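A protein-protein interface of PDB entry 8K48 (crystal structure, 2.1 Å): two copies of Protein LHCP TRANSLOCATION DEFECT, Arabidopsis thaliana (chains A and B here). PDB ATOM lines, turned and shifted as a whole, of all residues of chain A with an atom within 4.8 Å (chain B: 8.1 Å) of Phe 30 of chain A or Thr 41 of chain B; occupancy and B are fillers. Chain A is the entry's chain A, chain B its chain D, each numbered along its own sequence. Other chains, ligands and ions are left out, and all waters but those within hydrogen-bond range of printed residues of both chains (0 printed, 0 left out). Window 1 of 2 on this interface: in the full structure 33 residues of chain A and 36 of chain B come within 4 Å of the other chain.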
ATOM      1  N   VAL A  26     -19.887  -1.610  19.593  1.00  0.00           N
ATOM      2  CA  VAL A  26     -20.064  -0.366  20.352  1.00  0.00           C
ATOM      3  C   VAL A  26     -19.256  -0.410  21.639  1.00  0.00           C
ATOM      4  O   VAL A  26     -18.498   0.524  21.948  1.00  0.00           O
ATOM      5  CB  VAL A  26     -21.557  -0.112  20.635  1.00  0.00           C
ATOM      6  CG1 VAL A  26     -21.724   1.115  21.546  1.00  0.00           C
ATOM      7  CG2 VAL A  26     -22.328   0.083  19.329  1.00  0.00           C
ATOM      8  N   GLU A  27     -19.397  -1.503  22.384  1.00  0.00           N
ATOM      9  CA  GLU A  27     -18.700  -1.624  23.688  1.00  0.00           C
ATOM     10  C   GLU A  27     -17.179  -1.612  23.474  1.00  0.00           C
ATOM     11  O   GLU A  27     -16.479  -0.989  24.284  1.00  0.00           O
ATOM     12  CB  GLU A  27     -19.209  -2.870  24.414  1.00  0.00           C
ATOM     13  CG  GLU A  27     -20.571  -2.667  25.049  1.00  0.00           C
ATOM     14  CD  GLU A  27     -21.347  -3.943  25.321  1.00  0.00           C
ATOM     15  OE1 GLU A  27     -22.426  -3.854  25.936  1.00  0.00           O
ATOM     16  OE2 GLU A  27     -20.871  -5.019  24.919  1.00  0.00           O
ATOM     17  N   GLN A  28     -16.697  -2.297  22.436  1.00  0.00           N
ATOM     18  CA  GLN A  28     -15.236  -2.351  22.160  1.00  0.00           C
ATOM     19  C   GLN A  28     -14.692  -0.954  21.832  1.00  0.00           C
ATOM     20  O   GLN A  28     -13.617  -0.607  22.341  1.00  0.00           O
ATOM     21  CB  GLN A  28     -14.958  -3.319  21.009  1.00  0.00           C
ATOM     22  CG  GLN A  28     -14.987  -4.783  21.421  1.00  0.00           C
ATOM     23  CD  GLN A  28     -14.826  -5.706  20.237  1.00  0.00           C
ATOM     24  OE1 GLN A  28     -13.770  -6.296  20.023  1.00  0.00           O
ATOM     25  NE2 GLN A  28     -15.882  -5.835  19.451  1.00  0.00           N
ATOM     26  N   TYR A  29     -15.432  -0.180  21.038  1.00  0.00           N
ATOM     27  CA  TYR A  29     -14.972   1.176  20.658  1.00  0.00           C
ATOM     28  C   TYR A  29     -14.975   2.031  21.919  1.00  0.00           C
ATOM     29  O   TYR A  29     -14.009   2.772  22.150  1.00  0.00           O
ATOM     30  CB  TYR A  29     -15.864   1.798  19.584  1.00  0.00           C
ATOM     31  CG  TYR A  29     -15.417   3.164  19.129  1.00  0.00           C
ATOM     32  CD1 TYR A  29     -16.090   4.306  19.526  1.00  0.00           C
ATOM     33  CD2 TYR A  29     -14.310   3.316  18.312  1.00  0.00           C
ATOM     34  CE1 TYR A  29     -15.680   5.564  19.118  1.00  0.00           C
ATOM     35  CE2 TYR A  29     -13.889   4.566  17.892  1.00  0.00           C
ATOM     36  CZ  TYR A  29     -14.575   5.695  18.297  1.00  0.00           C
ATOM     37  OH  TYR A  29     -14.159   6.937  17.888  1.00  0.00           O
ATOM     38  N   PHE A  30     -16.033   1.899  22.711  1.00  0.00           N
ATOM     39  CA  PHE A  30     -16.058   2.621  23.977  1.00  0.00           C
ATOM     40  C   PHE A  30     -14.827   2.309  24.822  1.00  0.00           C
ATOM     41  O   PHE A  30     -14.157   3.220  25.326  1.00  0.00           O
ATOM     42  CB  PHE A  30     -17.329   2.277  24.749  1.00  0.00           C
ATOM     43  CG  PHE A  30     -17.465   3.038  26.030  1.00  0.00           C
ATOM     44  CD1 PHE A  30     -16.823   2.605  27.185  1.00  0.00           C
ATOM     45  CD2 PHE A  30     -18.204   4.214  26.073  1.00  0.00           C
ATOM     46  CE1 PHE A  30     -16.930   3.316  28.376  1.00  0.00           C
ATOM     47  CE2 PHE A  30     -18.317   4.935  27.261  1.00  0.00           C
ATOM     48  CZ  PHE A  30     -17.671   4.474  28.420  1.00  0.00           C
ATOM     49  N   ASN A  31     -14.527   1.022  25.014  1.00  0.00           N
ATOM     50  CA  ASN A  31     -13.402   0.654  25.866  1.00  0.00           C
ATOM     51  C   ASN A  31     -12.082   1.114  25.265  1.00  0.00           C
ATOM     52  O   ASN A  31     -11.197   1.587  25.987  1.00  0.00           O
ATOM     53  CB  ASN A  31     -13.394  -0.858  26.118  1.00  0.00           C
ATOM     54  CG  ASN A  31     -14.558  -1.324  27.016  1.00  0.00           C
ATOM     55  OD1 ASN A  31     -15.138  -0.537  27.775  1.00  0.00           O
ATOM     56  ND2 ASN A  31     -14.907  -2.601  26.912  1.00  0.00           N
ATOM     57  N   TYR A  32     -11.928   0.989  23.944  1.00  0.00           N
ATOM     58  CA  TYR A  32     -10.693   1.444  23.308  1.00  0.00           C
ATOM     59  C   TYR A  32     -10.498   2.939  23.492  1.00  0.00           C
ATOM     60  O   TYR A  32      -9.423   3.400  23.905  1.00  0.00           O
ATOM     61  CB  TYR A  32     -10.704   1.098  21.823  1.00  0.00           C
ATOM     62  CG  TYR A  32      -9.447   1.552  21.112  1.00  0.00           C
ATOM     63  CD1 TYR A  32      -9.482   2.594  20.188  1.00  0.00           C
ATOM     64  CD2 TYR A  32      -8.217   0.954  21.378  1.00  0.00           C
ATOM     65  CE1 TYR A  32      -8.321   3.016  19.531  1.00  0.00           C
ATOM     66  CE2 TYR A  32      -7.053   1.369  20.727  1.00  0.00           C
ATOM     67  CZ  TYR A  32      -7.110   2.397  19.807  1.00  0.00           C
ATOM     68  OH  TYR A  32      -5.955   2.805  19.158  1.00  0.00           O
ATOM     69  N   MET A  33     -11.521   3.726  23.174  1.00  0.00           N
ATOM     70  CA  MET A  33     -11.386   5.161  23.380  1.00  0.00           C
ATOM     71  C   MET A  33     -11.188   5.473  24.859  1.00  0.00           C
ATOM     72  O   MET A  33     -10.413   6.362  25.212  1.00  0.00           O
ATOM     73  CB  MET A  33     -12.600   5.892  22.799  1.00  0.00           C
ATOM     74  CG  MET A  33     -12.827   5.617  21.302  1.00  0.00           C
ATOM     75  SD  MET A  33     -11.378   5.871  20.223  1.00  0.00           S
ATOM     76  CE  MET A  33     -11.306   7.659  20.211  1.00  0.00           C
ATOM     77  N   GLY A  34     -11.862   4.737  25.743  1.00  0.00           N
ATOM     78  CA  GLY A  34     -11.608   4.913  27.162  1.00  0.00           C
ATOM     79  C   GLY A  34     -10.150   4.688  27.520  1.00  0.00           C
ATOM     80  O   GLY A  34      -9.576   5.420  28.332  1.00  0.00           O
ATOM     81  N   GLY B  34     -11.723  10.955  36.491  1.00  0.00           N
ATOM     82  CA  GLY B  34     -11.748  10.024  35.372  1.00  0.00           C
ATOM     83  C   GLY B  34     -12.745   8.900  35.575  1.00  0.00           C
ATOM     84  O   GLY B  34     -13.398   8.457  34.625  1.00  0.00           O
ATOM     85  N   MET B  35     -12.875   8.422  36.814  1.00  0.00           N
ATOM     86  CA  MET B  35     -13.870   7.401  37.122  1.00  0.00           C
ATOM     87  C   MET B  35     -15.283   7.930  36.896  1.00  0.00           C
ATOM     88  O   MET B  35     -16.108   7.264  36.266  1.00  0.00           O
ATOM     89  CB  MET B  35     -13.690   6.918  38.565  1.00  0.00           C
ATOM     90  CG  MET B  35     -14.707   5.871  39.018  1.00  0.00           C
ATOM     91  SD  MET B  35     -14.869   5.796  40.823  1.00  0.00           S
ATOM     92  CE  MET B  35     -15.741   7.337  41.139  1.00  0.00           C
ATOM     93  N   LEU B  36     -15.577   9.135  37.399  1.00  0.00           N
ATOM     94  CA  LEU B  36     -16.907   9.717  37.223  1.00  0.00           C
ATOM     95  C   LEU B  36     -17.253   9.877  35.746  1.00  0.00           C
ATOM     96  O   LEU B  36     -18.386   9.599  35.333  1.00  0.00           O
ATOM     97  CB  LEU B  36     -16.993  11.068  37.942  1.00  0.00           C
ATOM     98  CG  LEU B  36     -17.855  11.142  39.212  1.00  0.00           C
ATOM     99  CD1 LEU B  36     -17.185  10.420  40.359  1.00  0.00           C
ATOM    100  CD2 LEU B  36     -18.153  12.585  39.620  1.00  0.00           C
ATOM    101  N   ALA B  37     -16.287  10.322  34.940  1.00  0.00           N
ATOM    102  CA  ALA B  37     -16.493  10.431  33.498  1.00  0.00           C
ATOM    103  C   ALA B  37     -16.816   9.076  32.876  1.00  0.00           C
ATOM    104  O   ALA B  37     -17.838   8.917  32.202  1.00  0.00           O
ATOM    105  CB  ALA B  37     -15.251  11.032  32.845  1.00  0.00           C
ATOM    106  N   VAL B  38     -15.945   8.089  33.101  1.00  0.00           N
ATOM    107  CA  VAL B  38     -16.147   6.749  32.555  1.00  0.00           C
ATOM    108  C   VAL B  38     -17.502   6.203  32.976  1.00  0.00           C
ATOM    109  O   VAL B  38     -18.273   5.694  32.149  1.00  0.00           O
ATOM    110  CB  VAL B  38     -15.002   5.821  33.002  1.00  0.00           C
ATOM    111  CG1 VAL B  38     -15.364   4.353  32.762  1.00  0.00           C
ATOM    112  CG2 VAL B  38     -13.711   6.191  32.285  1.00  0.00           C
ATOM    113  N   GLU B  39     -17.829   6.315  34.268  1.00  0.00           N
ATOM    114  CA  GLU B  39     -19.056   5.693  34.749  1.00  0.00           C
ATOM    115  C   GLU B  39     -20.285   6.358  34.151  1.00  0.00           C
ATOM    116  O   GLU B  39     -21.277   5.677  33.863  1.00  0.00           O
ATOM    117  CB  GLU B  39     -19.106   5.710  36.281  1.00  0.00           C
ATOM    118  CG  GLU B  39     -17.991   4.853  36.921  1.00  0.00           C
ATOM    119  CD  GLU B  39     -18.099   4.698  38.434  1.00  0.00           C
ATOM    120  OE1 GLU B  39     -17.737   3.620  38.959  1.00  0.00           O
ATOM    121  OE2 GLU B  39     -18.539   5.654  39.102  1.00  0.00           O
ATOM    122  N   GLY B  40     -20.239   7.673  33.933  1.00  0.00           N
ATOM    123  CA  GLY B  40     -21.389   8.341  33.346  1.00  0.00           C
ATOM    124  C   GLY B  40     -21.582   7.950  31.895  1.00  0.00           C
ATOM    125  O   GLY B  40     -22.676   7.563  31.480  1.00  0.00           O
ATOM    126  N   THR B  41     -20.503   8.001  31.118  1.00  0.00           N
ATOM    127  CA  THR B  41     -20.592   7.690  29.696  1.00  0.00           C
ATOM    128  C   THR B  41     -20.858   6.207  29.453  1.00  0.00           C
ATOM    129  O   THR B  41     -21.615   5.856  28.540  1.00  0.00           O
ATOM    130  CB  THR B  41     -19.313   8.122  29.002  1.00  0.00           C
ATOM    131  OG1 THR B  41     -18.206   7.534  29.681  1.00  0.00           O
ATOM    132  CG2 THR B  41     -19.181   9.657  29.043  1.00  0.00           C
ATOM    133  N   TYR B  42     -20.235   5.322  30.245  1.00  0.00           N
ATOM    134  CA  TYR B  42     -20.533   3.894  30.126  1.00  0.00           C
ATOM    135  C   TYR B  42     -22.025   3.641  30.287  1.00  0.00           C
ATOM    136  O   TYR B  42     -22.647   2.986  29.446  1.00  0.00           O
ATOM    137  CB  TYR B  42     -19.736   3.078  31.157  1.00  0.00           C
ATOM    138  CG  TYR B  42     -19.995   1.580  31.065  1.00  0.00           C
ATOM    139  CD1 TYR B  42     -20.890   0.945  31.928  1.00  0.00           C
ATOM    140  CD2 TYR B  42     -19.366   0.804  30.089  1.00  0.00           C
ATOM    141  CE1 TYR B  42     -21.141  -0.433  31.829  1.00  0.00           C
ATOM    142  CE2 TYR B  42     -19.590  -0.553  29.992  1.00  0.00           C
ATOM    143  CZ  TYR B  42     -20.479  -1.178  30.862  1.00  0.00           C
ATOM    144  OH  TYR B  42     -20.715  -2.544  30.744  1.00  0.00           O
ATOM    145  N   SER B  43     -22.621   4.176  31.359  1.00  0.00           N
ATOM    146  CA  SER B  43     -24.042   3.941  31.617  1.00  0.00           C
ATOM    147  C   SER B  43     -24.920   4.503  30.508  1.00  0.00           C
ATOM    148  O   SER B  43     -25.883   3.856  30.079  1.00  0.00           O
ATOM    149  CB  SER B  43     -24.435   4.545  32.964  1.00  0.00           C
ATOM    150  OG  SER B  43     -23.991   3.697  34.010  1.00  0.00           O
ATOM    151  N   LYS B  44     -24.610   5.704  30.034  1.00  0.00           N
ATOM    152  CA  LYS B  44     -25.378   6.285  28.942  1.00  0.00           C
ATOM    153  C   LYS B  44     -25.281   5.412  27.697  1.00  0.00           C
ATOM    154  O   LYS B  44     -26.290   5.134  27.035  1.00  0.00           O
ATOM    155  CB  LYS B  44     -24.877   7.706  28.668  1.00  0.00           C
ATOM    156  CG  LYS B  44     -25.286   8.731  29.764  1.00  0.00           C
ATOM    157  CD  LYS B  44     -25.504  10.131  29.188  1.00  0.00           C
ATOM    158  CE  LYS B  44     -26.727  10.828  29.800  1.00  0.00           C
ATOM    159  NZ  LYS B  44     -27.753  11.150  28.763  1.00  0.00           N
ATOM    160  N   MET B  45     -24.066   4.948  27.386  1.00  0.00           N
ATOM    161  CA  MET B  45     -23.852   4.081  26.232  1.00  0.00           C
ATOM    162  C   MET B  45     -24.685   2.813  26.351  1.00  0.00           C
ATOM    163  O   MET B  45     -25.411   2.449  25.419  1.00  0.00           O
ATOM    164  CB  MET B  45     -22.354   3.769  26.107  1.00  0.00           C
ATOM    165  CG  MET B  45     -21.936   2.882  24.930  1.00  0.00           C
ATOM    166  SD  MET B  45     -21.782   1.181  25.477  1.00  0.00           S
ATOM    167  CE  MET B  45     -20.458   1.263  26.712  1.00  0.00           C
ATOM    168  N   GLU B  46     -24.625   2.148  27.508  1.00  0.00           N
ATOM    169  CA  GLU B  46     -25.393   0.919  27.701  1.00  0.00           C
ATOM    170  C   GLU B  46     -26.900   1.156  27.594  1.00  0.00           C
ATOM    171  O   GLU B  46     -27.631   0.287  27.097  1.00  0.00           O
ATOM    172  CB  GLU B  46     -25.053   0.293  29.055  1.00  0.00           C
ATOM    173  CG  GLU B  46     -23.639  -0.265  29.137  1.00  0.00           C
ATOM    174  CD  GLU B  46     -23.400  -1.421  28.178  1.00  0.00           C
ATOM    175  OE1 GLU B  46     -22.406  -1.389  27.430  1.00  0.00           O
ATOM    176  OE2 GLU B  46     -24.200  -2.369  28.165  1.00  0.00           O
ATOM    177  N   ALA B  47     -27.383   2.319  28.048  1.00  0.00           N
ATOM    178  CA  ALA B  47     -28.809   2.604  27.947  1.00  0.00           C
ATOM    179  C   ALA B  47     -29.232   2.732  26.489  1.00  0.00           C
ATOM    180  O   ALA B  47     -30.268   2.190  26.091  1.00  0.00           O
ATOM    181  CB  ALA B  47     -29.153   3.874  28.727  1.00  0.00           C
ATOM    182  N   LEU B  48     -28.420   3.430  25.678  1.00  0.00           N
ATOM    183  CA  LEU B  48     -28.676   3.549  24.238  1.00  0.00           C
ATOM    184  C   LEU B  48     -28.773   2.190  23.571  1.00  0.00           C
ATOM    185  O   LEU B  48     -29.647   1.970  22.727  1.00  0.00           O
ATOM    186  CB  LEU B  48     -27.569   4.356  23.568  1.00  0.00           C
ATOM    187  CG  LEU B  48     -27.476   5.814  23.976  1.00  0.00           C
ATOM    188  CD1 LEU B  48     -26.251   6.458  23.338  1.00  0.00           C
ATOM    189  CD2 LEU B  48     -28.771   6.526  23.587  1.00  0.00           C
ATOM    190  N   LEU B  49     -27.864   1.275  23.920  1.00  0.00           N
ATOM    191  CA  LEU B  49     -27.932  -0.092  23.418  1.00  0.00           C
ATOM    192  C   LEU B  49     -29.253  -0.757  23.807  1.00  0.00           C
ATOM    193  O   LEU B  49     -29.930  -1.359  22.967  1.00  0.00           O
ATOM    194  CB  LEU B  49     -26.738  -0.888  23.950  1.00  0.00           C
ATOM    195  CG  LEU B  49     -25.396  -0.612  23.262  1.00  0.00           C
ATOM    196  CD1 LEU B  49     -24.263  -1.237  24.057  1.00  0.00           C
ATOM    197  CD2 LEU B  49     -25.409  -1.128  21.824  1.00  0.00           C
ATOM    198  N   ILE B  58     -25.149   4.372  17.104  1.00  0.00           N
ATOM    199  CA  ILE B  58     -24.500   4.686  18.376  1.00  0.00           C
ATOM    200  C   ILE B  58     -23.015   4.913  18.158  1.00  0.00           C
ATOM    201  O   ILE B  58     -22.415   5.826  18.742  1.00  0.00           O
ATOM    202  CB  ILE B  58     -24.763   3.568  19.411  1.00  0.00           C
ATOM    203  CG1 ILE B  58     -26.270   3.348  19.591  1.00  0.00           C
ATOM    204  CG2 ILE B  58     -24.130   3.928  20.739  1.00  0.00           C
ATOM    205  CD1 ILE B  58     -26.636   2.231  20.599  1.00  0.00           C
ATOM    206  N   LEU B  59     -22.400   4.103  17.289  1.00  0.00           N
ATOM    207  CA  LEU B  59     -20.977   4.263  17.007  1.00  0.00           C
ATOM    208  C   LEU B  59     -20.682   5.619  16.385  1.00  0.00           C
ATOM    209  O   LEU B  59     -19.634   6.217  16.652  1.00  0.00           O
ATOM    210  CB  LEU B  59     -20.487   3.139  16.095  1.00  0.00           C
ATOM    211  CG  LEU B  59     -20.097   1.876  16.869  1.00  0.00           C
ATOM    212  CD1 LEU B  59     -20.240   0.633  16.002  1.00  0.00           C
ATOM    213  CD2 LEU B  59     -18.688   1.994  17.401  1.00  0.00           C
ATOM    214  N   LEU B  62     -20.622   8.141  19.210  1.00  0.00           N
ATOM    215  CA  LEU B  62     -19.382   8.075  19.981  1.00  0.00           C
ATOM    216  C   LEU B  62     -18.209   8.623  19.184  1.00  0.00           C
ATOM    217  O   LEU B  62     -17.408   9.403  19.709  1.00  0.00           O
ATOM    218  CB  LEU B  62     -19.091   6.632  20.405  1.00  0.00           C
ATOM    219  CG  LEU B  62     -20.152   5.976  21.280  1.00  0.00           C
ATOM    220  CD1 LEU B  62     -19.821   4.510  21.517  1.00  0.00           C
ATOM    221  CD2 LEU B  62     -20.261   6.731  22.599  1.00  0.00           C
ATOM    222  N   THR B  65     -18.361  12.372  19.176  1.00  0.00           N
ATOM    223  CA  THR B  65     -17.866  12.905  20.442  1.00  0.00           C
ATOM    224  C   THR B  65     -16.343  12.920  20.470  1.00  0.00           C
ATOM    225  O   THR B  65     -15.731  13.883  20.943  1.00  0.00           O
ATOM    226  CB  THR B  65     -18.417  12.081  21.614  1.00  0.00           C
ATOM    227  OG1 THR B  65     -19.829  12.284  21.731  1.00  0.00           O
ATOM    228  CG2 THR B  65     -17.749  12.479  22.921  1.00  0.00           C
ATOM    229  N   GLU B  66     -15.717  11.877  19.927  1.00  0.00           N
ATOM    230  CA  GLU B  66     -14.263  11.758  19.941  1.00  0.00           C
ATOM    231  C   GLU B  66     -13.579  12.534  18.829  1.00  0.00           C
ATOM    232  O   GLU B  66     -12.347  12.623  18.836  1.00  0.00           O
ATOM    233  CB  GLU B  66     -13.841  10.291  19.819  1.00  0.00           C
ATOM    234  CG  GLU B  66     -14.376   9.387  20.895  1.00  0.00           C
ATOM    235  CD  GLU B  66     -13.626   9.542  22.202  1.00  0.00           C
ATOM    236  OE1 GLU B  66     -12.484  10.055  22.186  1.00  0.00           O
ATOM    237  OE2 GLU B  66     -14.183   9.149  23.244  1.00  0.00           O
ATOM    238  N   ARG B  95     -23.146  16.166  19.028  1.00  0.00           N
ATOM    239  CA  ARG B  95     -22.034  15.644  19.814  1.00  0.00           C
ATOM    240  C   ARG B  95     -20.679  16.026  19.232  1.00  0.00           C
ATOM    241  O   ARG B  95     -19.669  15.927  19.934  1.00  0.00           O
ATOM    242  CB  ARG B  95     -22.134  14.120  19.913  1.00  0.00           C
ATOM    243  CG  ARG B  95     -23.376  13.600  20.610  1.00  0.00           C
ATOM    244  CD  ARG B  95     -23.414  12.073  20.518  1.00  0.00           C
ATOM    245  NE  ARG B  95     -24.066  11.442  21.658  1.00  0.00           N
ATOM    246  CZ  ARG B  95     -23.429  10.754  22.606  1.00  0.00           C
ATOM    247  NH1 ARG B  95     -24.127  10.218  23.596  1.00  0.00           N
ATOM    248  NH2 ARG B  95     -22.100  10.593  22.565  1.00  0.00           N
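O of Glu 27 of chain A sits close to ND2 of Asn 31 of chain A (3.5 Å). The side-chain hydroxyl (OH) of Tyr 29 of chain A lies close to the side-chain sulfur (SD) of Met 33 of chain A (3.8 Å). OG1 of Thr 41 of chain B is in hydrogen-bond range of O of Ala 37 of chain B. The backbone carbonyl oxygen (O) of Val 38 of chain B sits at hydrogen-bond distance from the side-chain hydroxyl (OG1) of Thr 41 of chain B, at 3.1 Å.
Of the 9 printed residues of chain A, 5 touch a printed residue of chain B. Hydrophobic or aromatic side chains of chain B within 4 Å of the printed part of chain A: Tyr 42, Met 45, Leu 49, Ile 58, Leu 59 and Leu 62. Among the printed residues, no Asp or Glu carboxylate lies within 4 Å of a Lys or Arg side-chain nitrogen of the other chain.
Printed residues of chain B within 4 Å of Tyr 29 of chain A: Leu 59, Leu 62 and Glu 66. Phe 30 of chain A touches four residues of chain B. Of the printed residues of chain A, Val 38 of chain B touches Phe 30. Of chain A, only Phe 30 comes within 4 Å of Thr 41 of chain B. Ala 47 of chain B touches none of the printed residues of chain A. Printed residues of chain A within 4 Å of Leu 49 of chain B: Glu 27 (3.7 Å). Printed residues of chain A within 4 Å of Leu 59 of chain B: Val 26 (3.8 Å) and Tyr 29 (3.6 Å). Printed residues of chain A within 4 Å of Leu 62 of chain B: Val 26 (3.9 Å) and Tyr 29 (3.8 Å). The nearest residue of chain B that does not touch Phe 30 of chain A is Leu 62 of chain B (4.7 Å). The nearest printed residue of chain A that does not touch Thr 41 of chain B is Gly 34 of chain A (7.5 Å).
1 position is printed for both chains.
Among the printed residues, merely in contact across the chains: Val 26 of chain A with Met 45 of chain B (3.8 Å), Val 26 of chain A with Ile 58 of chain B (3.8 Å), Val 26 of chain A with Leu 59 of chain B (3.8 Å), Val 26 of chain A with Leu 62 of chain B (3.9 Å), Glu 27 of chain A with Leu 49 of chain B (3.7 Å), Tyr 29 of chain A with Leu 59 of chain B (3.6 Å), Tyr 29 of chain A with Leu 62 of chain B (3.8 Å), Tyr 29 of chain A with Glu 66 of chain B (3.9 Å), Phe 30 of chain A with Val 38 of chain B (3.97 Å), Phe 30 of chain A with Thr 41 of chain B (3.4 Å), Phe 30 of chain A with Tyr 42 of chain B (3.3 Å), Phe 30 of chain A with Met 45 of chain B (3.5 Å) and Met 33 of chain A with Glu 66 of chain B (3.3 Å).
OE1 of Glu 46 of chain B sits close to OE1 of Glu 27 of chain A (2.9 Å).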
